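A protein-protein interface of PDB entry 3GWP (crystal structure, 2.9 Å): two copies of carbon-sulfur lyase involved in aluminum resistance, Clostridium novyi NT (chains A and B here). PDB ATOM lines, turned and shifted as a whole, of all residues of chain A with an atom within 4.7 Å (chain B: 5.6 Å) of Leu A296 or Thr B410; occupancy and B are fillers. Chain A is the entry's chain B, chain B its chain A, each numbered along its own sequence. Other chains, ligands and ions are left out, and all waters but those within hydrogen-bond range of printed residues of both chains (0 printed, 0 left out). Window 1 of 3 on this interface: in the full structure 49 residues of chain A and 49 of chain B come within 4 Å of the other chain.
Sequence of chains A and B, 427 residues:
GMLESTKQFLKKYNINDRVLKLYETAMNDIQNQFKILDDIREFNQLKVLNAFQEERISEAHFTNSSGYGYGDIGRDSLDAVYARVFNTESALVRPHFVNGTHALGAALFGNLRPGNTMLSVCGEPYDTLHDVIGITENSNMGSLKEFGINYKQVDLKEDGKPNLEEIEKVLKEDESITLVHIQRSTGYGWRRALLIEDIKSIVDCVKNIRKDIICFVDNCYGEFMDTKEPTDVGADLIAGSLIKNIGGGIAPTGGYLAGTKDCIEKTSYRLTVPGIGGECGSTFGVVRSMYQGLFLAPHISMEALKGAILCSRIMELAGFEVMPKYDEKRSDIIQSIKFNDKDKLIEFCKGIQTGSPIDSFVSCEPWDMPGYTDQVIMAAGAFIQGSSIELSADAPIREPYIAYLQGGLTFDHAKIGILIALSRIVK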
ATOM      1  N   GLN A  45     -14.073  -4.735   5.991  1.00  0.00           N
ATOM      2  CA  GLN A  45     -14.796  -3.785   6.826  1.00  0.00           C
ATOM      3  C   GLN A  45     -15.763  -3.008   5.924  1.00  0.00           C
ATOM      4  O   GLN A  45     -16.942  -2.852   6.257  1.00  0.00           O
ATOM      5  CB  GLN A  45     -13.830  -2.824   7.545  1.00  0.00           C
ATOM      6  CG  GLN A  45     -14.516  -1.847   8.514  1.00  0.00           C
ATOM      7  CD  GLN A  45     -15.179  -2.548   9.685  1.00  0.00           C
ATOM      8  OE1 GLN A  45     -14.513  -3.166  10.510  1.00  0.00           O
ATOM      9  NE2 GLN A  45     -16.489  -2.407   9.791  1.00  0.00           N
ATOM     10  N   GLY A 248     -17.724 -11.936  15.921  1.00  0.00           N
ATOM     11  CA  GLY A 248     -16.873 -10.851  16.413  1.00  0.00           C
ATOM     12  C   GLY A 248     -16.663 -10.811  17.916  1.00  0.00           C
ATOM     13  O   GLY A 248     -16.432  -9.750  18.471  1.00  0.00           O
ATOM     14  N   ILE A 250     -18.802 -10.951  20.233  1.00  0.00           N
ATOM     15  CA  ILE A 250     -20.000 -10.447  20.916  1.00  0.00           C
ATOM     16  C   ILE A 250     -21.169 -11.439  20.831  1.00  0.00           C
ATOM     17  O   ILE A 250     -21.891 -11.632  21.819  1.00  0.00           O
ATOM     18  CB  ILE A 250     -20.476  -9.120  20.298  1.00  0.00           C
ATOM     19  CG1 ILE A 250     -19.400  -8.052  20.408  1.00  0.00           C
ATOM     20  CG2 ILE A 250     -21.733  -8.631  20.983  1.00  0.00           C
ATOM     21  CD1 ILE A 250     -19.861  -6.695  19.858  1.00  0.00           C
ATOM     22  N   GLN A 292     -23.986  -6.126  15.453  1.00  0.00           N
ATOM     23  CA  GLN A 292     -22.746  -5.507  15.925  1.00  0.00           C
ATOM     24  C   GLN A 292     -21.580  -6.489  15.843  1.00  0.00           C
ATOM     25  O   GLN A 292     -20.446  -6.100  15.530  1.00  0.00           O
ATOM     26  CB  GLN A 292     -22.922  -5.001  17.357  1.00  0.00           C
ATOM     27  CG  GLN A 292     -21.770  -4.147  17.866  1.00  0.00           C
ATOM     28  CD  GLN A 292     -22.063  -3.529  19.209  1.00  0.00           C
ATOM     29  OE1 GLN A 292     -22.966  -3.966  19.925  1.00  0.00           O
ATOM     30  NE2 GLN A 292     -21.305  -2.501  19.561  1.00  0.00           N
ATOM     31  N   GLY A 293     -21.865  -7.759  16.129  1.00  0.00           N
ATOM     32  CA  GLY A 293     -20.867  -8.810  16.048  1.00  0.00           C
ATOM     33  C   GLY A 293     -20.336  -8.962  14.635  1.00  0.00           C
ATOM     34  O   GLY A 293     -19.128  -9.117  14.431  1.00  0.00           O
ATOM     35  N   LEU A 294     -21.244  -8.927  13.659  1.00  0.00           N
ATOM     36  CA  LEU A 294     -20.866  -9.027  12.258  1.00  0.00           C
ATOM     37  C   LEU A 294     -20.015  -7.837  11.890  1.00  0.00           C
ATOM     38  O   LEU A 294     -18.938  -7.996  11.320  1.00  0.00           O
ATOM     39  CB  LEU A 294     -22.111  -9.087  11.358  1.00  0.00           C
ATOM     40  CG  LEU A 294     -21.895  -9.100   9.838  1.00  0.00           C
ATOM     41  CD1 LEU A 294     -21.028 -10.269   9.423  1.00  0.00           C
ATOM     42  CD2 LEU A 294     -23.240  -9.136   9.123  1.00  0.00           C
ATOM     43  N   PHE A 295     -20.474  -6.646  12.270  1.00  0.00           N
ATOM     44  CA  PHE A 295     -19.752  -5.412  11.971  1.00  0.00           C
ATOM     45  C   PHE A 295     -18.306  -5.416  12.524  1.00  0.00           C
ATOM     46  O   PHE A 295     -17.394  -4.895  11.873  1.00  0.00           O
ATOM     47  CB  PHE A 295     -20.524  -4.199  12.496  1.00  0.00           C
ATOM     48  CG  PHE A 295     -19.941  -2.893  12.073  1.00  0.00           C
ATOM     49  CD1 PHE A 295     -20.143  -2.426  10.787  1.00  0.00           C
ATOM     50  CD2 PHE A 295     -19.191  -2.127  12.951  1.00  0.00           C
ATOM     51  CE1 PHE A 295     -19.606  -1.243  10.383  1.00  0.00           C
ATOM     52  CE2 PHE A 295     -18.653  -0.929  12.550  1.00  0.00           C
ATOM     53  CZ  PHE A 295     -18.861  -0.487  11.265  1.00  0.00           C
ATOM     54  N   LEU A 296     -18.109  -6.012  13.711  1.00  0.00           N
ATOM     55  CA  LEU A 296     -16.765  -6.125  14.322  1.00  0.00           C
ATOM     56  C   LEU A 296     -15.974  -7.353  13.829  1.00  0.00           C
ATOM     57  O   LEU A 296     -14.760  -7.421  14.032  1.00  0.00           O
ATOM     58  CB  LEU A 296     -16.864  -6.182  15.854  1.00  0.00           C
ATOM     59  CG  LEU A 296     -17.285  -4.905  16.587  1.00  0.00           C
ATOM     60  CD1 LEU A 296     -17.546  -5.201  18.043  1.00  0.00           C
ATOM     61  CD2 LEU A 296     -16.226  -3.831  16.447  1.00  0.00           C
ATOM     62  N   ALA A 297     -16.661  -8.301  13.176  1.00  0.00           N
ATOM     63  CA  ALA A 297     -16.038  -9.562  12.705  1.00  0.00           C
ATOM     64  C   ALA A 297     -14.745  -9.402  11.896  1.00  0.00           C
ATOM     65  O   ALA A 297     -13.737  -9.998  12.252  1.00  0.00           O
ATOM     66  CB  ALA A 297     -17.055 -10.408  11.928  1.00  0.00           C
ATOM     67  N   PRO A 298     -14.773  -8.612  10.798  1.00  0.00           N
ATOM     68  CA  PRO A 298     -13.548  -8.433  10.010  1.00  0.00           C
ATOM     69  C   PRO A 298     -12.345  -7.948  10.827  1.00  0.00           C
ATOM     70  O   PRO A 298     -11.218  -8.360  10.562  1.00  0.00           O
ATOM     71  CB  PRO A 298     -13.947  -7.376   8.980  1.00  0.00           C
ATOM     72  CG  PRO A 298     -15.397  -7.522   8.838  1.00  0.00           C
ATOM     73  CD  PRO A 298     -15.907  -7.892  10.193  1.00  0.00           C
ATOM     74  N   HIS A 299     -12.595  -7.102  11.820  1.00  0.00           N
ATOM     75  CA  HIS A 299     -11.533  -6.580  12.662  1.00  0.00           C
ATOM     76  C   HIS A 299     -11.052  -7.622  13.674  1.00  0.00           C
ATOM     77  O   HIS A 299      -9.860  -7.939  13.722  1.00  0.00           O
ATOM     78  CB  HIS A 299     -11.994  -5.315  13.397  1.00  0.00           C
ATOM     79  CG  HIS A 299     -10.908  -4.651  14.183  1.00  0.00           C
ATOM     80  ND1 HIS A 299     -10.042  -3.736  13.627  1.00  0.00           N
ATOM     81  CD2 HIS A 299     -10.531  -4.788  15.475  1.00  0.00           C
ATOM     82  CE1 HIS A 299      -9.182  -3.333  14.544  1.00  0.00           C
ATOM     83  NE2 HIS A 299      -9.454  -3.959  15.673  1.00  0.00           N
ATOM     84  N   ILE A 300     -11.985  -8.161  14.461  1.00  0.00           N
ATOM     85  CA  ILE A 300     -11.657  -9.155  15.508  1.00  0.00           C
ATOM     86  C   ILE A 300     -11.006 -10.429  14.941  1.00  0.00           C
ATOM     87  O   ILE A 300     -10.128 -11.008  15.575  1.00  0.00           O
ATOM     88  CB  ILE A 300     -12.920  -9.536  16.368  1.00  0.00           C
ATOM     89  CG1 ILE A 300     -13.478  -8.304  17.118  1.00  0.00           C
ATOM     90  CG2 ILE A 300     -12.589 -10.639  17.374  1.00  0.00           C
ATOM     91  CD1 ILE A 300     -12.514  -7.687  18.137  1.00  0.00           C
ATOM     92  N   ILE B 250     -19.457  -2.072  23.759  1.00  0.00           N
ATOM     93  CA  ILE B 250     -20.318  -3.224  24.084  1.00  0.00           C
ATOM     94  C   ILE B 250     -21.298  -2.914  25.220  1.00  0.00           C
ATOM     95  O   ILE B 250     -22.464  -3.322  25.162  1.00  0.00           O
ATOM     96  CB  ILE B 250     -19.467  -4.463  24.481  1.00  0.00           C
ATOM     97  CG1 ILE B 250     -18.641  -4.942  23.295  1.00  0.00           C
ATOM     98  CG2 ILE B 250     -20.347  -5.598  24.951  1.00  0.00           C
ATOM     99  CD1 ILE B 250     -17.911  -6.232  23.559  1.00  0.00           C
ATOM    100  N   ILE B 300     -10.302  -0.882  21.966  1.00  0.00           N
ATOM    101  CA  ILE B 300     -11.305  -0.042  21.263  1.00  0.00           C
ATOM    102  C   ILE B 300     -11.051   1.465  21.405  1.00  0.00           C
ATOM    103  O   ILE B 300     -11.297   2.227  20.466  1.00  0.00           O
ATOM    104  CB  ILE B 300     -12.777  -0.378  21.727  1.00  0.00           C
ATOM    105  CG1 ILE B 300     -13.160  -1.805  21.318  1.00  0.00           C
ATOM    106  CG2 ILE B 300     -13.775   0.595  21.120  1.00  0.00           C
ATOM    107  CD1 ILE B 300     -13.211  -2.031  19.813  1.00  0.00           C
ATOM    108  N   GLU B 303      -8.644   2.563  18.795  1.00  0.00           N
ATOM    109  CA  GLU B 303      -9.187   2.498  17.432  1.00  0.00           C
ATOM    110  C   GLU B 303      -9.828   3.852  17.109  1.00  0.00           C
ATOM    111  O   GLU B 303      -9.661   4.381  16.013  1.00  0.00           O
ATOM    112  CB  GLU B 303     -10.221   1.371  17.292  1.00  0.00           C
ATOM    113  CG  GLU B 303      -9.662  -0.048  17.493  1.00  0.00           C
ATOM    114  CD  GLU B 303      -8.691  -0.484  16.404  1.00  0.00           C
ATOM    115  OE1 GLU B 303      -8.899  -0.127  15.227  1.00  0.00           O
ATOM    116  OE2 GLU B 303      -7.754  -1.242  16.722  1.00  0.00           O
ATOM    117  N   GLY B 408     -15.062   5.420  16.809  1.00  0.00           N
ATOM    118  CA  GLY B 408     -14.774   4.529  15.701  1.00  0.00           C
ATOM    119  C   GLY B 408     -14.397   3.178  16.284  1.00  0.00           C
ATOM    120  O   GLY B 408     -13.251   2.984  16.697  1.00  0.00           O
ATOM    121  N   LEU B 409     -15.374   2.258  16.352  1.00  0.00           N
ATOM    122  CA  LEU B 409     -15.159   0.898  16.921  1.00  0.00           C
ATOM    123  C   LEU B 409     -13.873   0.262  16.397  1.00  0.00           C
ATOM    124  O   LEU B 409     -13.106  -0.312  17.163  1.00  0.00           O
ATOM    125  CB  LEU B 409     -16.367  -0.015  16.648  1.00  0.00           C
ATOM    126  CG  LEU B 409     -17.710   0.367  17.314  1.00  0.00           C
ATOM    127  CD1 LEU B 409     -18.836  -0.519  16.807  1.00  0.00           C
ATOM    128  CD2 LEU B 409     -17.613   0.293  18.819  1.00  0.00           C
ATOM    129  N   THR B 410     -13.651   0.375  15.091  1.00  0.00           N
ATOM    130  CA  THR B 410     -12.423  -0.098  14.454  1.00  0.00           C
ATOM    131  C   THR B 410     -11.899   1.060  13.638  1.00  0.00           C
ATOM    132  O   THR B 410     -12.689   1.836  13.093  1.00  0.00           O
ATOM    133  CB  THR B 410     -12.666  -1.290  13.524  1.00  0.00           C
ATOM    134  OG1 THR B 410     -13.407  -0.868  12.368  1.00  0.00           O
ATOM    135  CG2 THR B 410     -13.420  -2.386  14.250  1.00  0.00           C
ATOM    136  N   PHE B 411     -10.574   1.190  13.566  1.00  0.00           N
ATOM    137  CA  PHE B 411      -9.937   2.276  12.809  1.00  0.00           C
ATOM    138  C   PHE B 411     -10.363   2.290  11.338  1.00  0.00           C
ATOM    139  O   PHE B 411     -10.538   3.365  10.750  1.00  0.00           O
ATOM    140  CB  PHE B 411      -8.416   2.187  12.919  1.00  0.00           C
ATOM    141  CG  PHE B 411      -7.694   3.162  12.043  1.00  0.00           C
ATOM    142  CD1 PHE B 411      -7.707   4.512  12.336  1.00  0.00           C
ATOM    143  CD2 PHE B 411      -6.990   2.730  10.928  1.00  0.00           C
ATOM    144  CE1 PHE B 411      -7.044   5.415  11.526  1.00  0.00           C
ATOM    145  CE2 PHE B 411      -6.320   3.632  10.118  1.00  0.00           C
ATOM    146  CZ  PHE B 411      -6.347   4.970  10.419  1.00  0.00           C
ATOM    147  N   ASP B 412     -10.537   1.103  10.754  1.00  0.00           N
ATOM    148  CA  ASP B 412     -10.966   0.987   9.362  1.00  0.00           C
ATOM    149  C   ASP B 412     -12.296   1.697   9.130  1.00  0.00           C
ATOM    150  O   ASP B 412     -12.434   2.434   8.169  1.00  0.00           O
ATOM    151  CB  ASP B 412     -11.059  -0.482   8.938  1.00  0.00           C
ATOM    152  CG  ASP B 412      -9.689  -1.148   8.810  1.00  0.00           C
ATOM    153  OD1 ASP B 412      -8.859  -0.670   8.008  1.00  0.00           O
ATOM    154  OD2 ASP B 412      -9.476  -2.190   9.462  1.00  0.00           O
ATOM    155  N   HIS B 413     -13.260   1.497  10.027  1.00  0.00           N
ATOM    156  CA  HIS B 413     -14.561   2.168   9.906  1.00  0.00           C
ATOM    157  C   HIS B 413     -14.424   3.677  10.056  1.00  0.00           C
ATOM    158  O   HIS B 413     -15.063   4.439   9.325  1.00  0.00           O
ATOM    159  CB  HIS B 413     -15.551   1.642  10.930  1.00  0.00           C
ATOM    160  CG  HIS B 413     -16.827   2.417  10.975  1.00  0.00           C
ATOM    161  ND1 HIS B 413     -17.285   3.030  12.120  1.00  0.00           N
ATOM    162  CD2 HIS B 413     -17.691   2.764   9.991  1.00  0.00           C
ATOM    163  CE1 HIS B 413     -18.415   3.658  11.855  1.00  0.00           C
ATOM    164  NE2 HIS B 413     -18.677   3.523  10.568  1.00  0.00           N
ATOM    165  N   ALA B 414     -13.601   4.103  11.010  1.00  0.00           N
ATOM    166  CA  ALA B 414     -13.360   5.518  11.244  1.00  0.00           C
ATOM    167  C   ALA B 414     -12.877   6.200   9.971  1.00  0.00           C
ATOM    168  O   ALA B 414     -13.459   7.191   9.548  1.00  0.00           O
ATOM    169  CB  ALA B 414     -12.341   5.708  12.371  1.00  0.00           C
ATOM    170  N   LYS B 415     -11.854   5.627   9.329  1.00  0.00           N
ATOM    171  CA  LYS B 415     -11.300   6.222   8.100  1.00  0.00           C
ATOM    172  C   LYS B 415     -12.267   6.146   6.908  1.00  0.00           C
ATOM    173  O   LYS B 415     -12.192   6.986   6.009  1.00  0.00           O
ATOM    174  CB  LYS B 415      -9.913   5.631   7.741  1.00  0.00           C
ATOM    175  CG  LYS B 415      -9.877   4.207   7.261  1.00  0.00           C
ATOM    176  CD  LYS B 415      -8.442   3.800   6.875  1.00  0.00           C
ATOM    177  CE  LYS B 415      -8.347   2.308   6.573  1.00  0.00           C
ATOM    178  NZ  LYS B 415      -6.973   1.865   6.246  1.00  0.00           N
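Among the printed residues, merely in contact across the chains: His A299 with Thr B410, Phe A295 with His B413, Gln A45 with Asp B412, Leu A296 with Leu B409, Leu A296 with Thr B410, Gln A45 with His B413 and Ile A250 with Ile B250.
OE1 of Glu B303 sits at hydrogen-bond distance from N of Phe B411, 2.7 Å away.
OG1 of Thr B410 lies within hydrogen-bond range of N of His B413 (3.3 Å).
OD1 of Asp B412 is in salt-bridge range of NZ of Lys B415, at 3.6 Å.
NE2 of Gln A45 lies within hydrogen-bond range of O of Phe A295 (3.4 Å).
A ring nitrogen (NE2) of His A299 lies close to the side-chain carboxylate (OE2) of Glu B303 (3.4 Å).
The side-chain amide oxygen (OE1) of Gln A45 lies within hydrogen-bond range of the side-chain hydroxyl (OG1) of Thr B410 (3.2 Å).
Ile A250 touches its own counterpart, Ile B250.
2 positions are printed for both chains.
Of the 9 pairs that touch across the chains among the printed residues, 1 has its exchanged pair printed and touching as well.
Of the 11 printed residues of chain B, 6 touch a printed residue of chain A.
Of the 12 printed residues of chain A, 5 touch a printed residue of chain B.
Hydrophobic or aromatic side chains of chain A within 4 Å of the printed part of chain B: Ile A250, Phe A295, Leu A296 and His A299.
Among the printed residues, 9 pairs touch across the chains.
Among the printed residues, no Asp or Glu carboxylate lies within 4 Å of a Lys or Arg side-chain nitrogen of the other chain.
Leu A296 touches just these residues of chain B: Leu B409 (3.8 Å) and Thr B410 (3.8 Å).
Of chain A, only Gln A45, Leu A296 and His A299 come within 4 Å of Thr B410.
Of the printed residues of chain B, His A299 touches Glu B303 (3.3 Å) and Thr B410 (3.4 Å).
Of the printed residues of chain A, Glu B303 touches His A299.
Of the printed residues of chain B, Phe A295 touches His B413 (3.6 Å).
Of the printed residues of chain A, Ile B250 touches Ile A250.
Lys B415 touches none of the printed residues of chain A.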
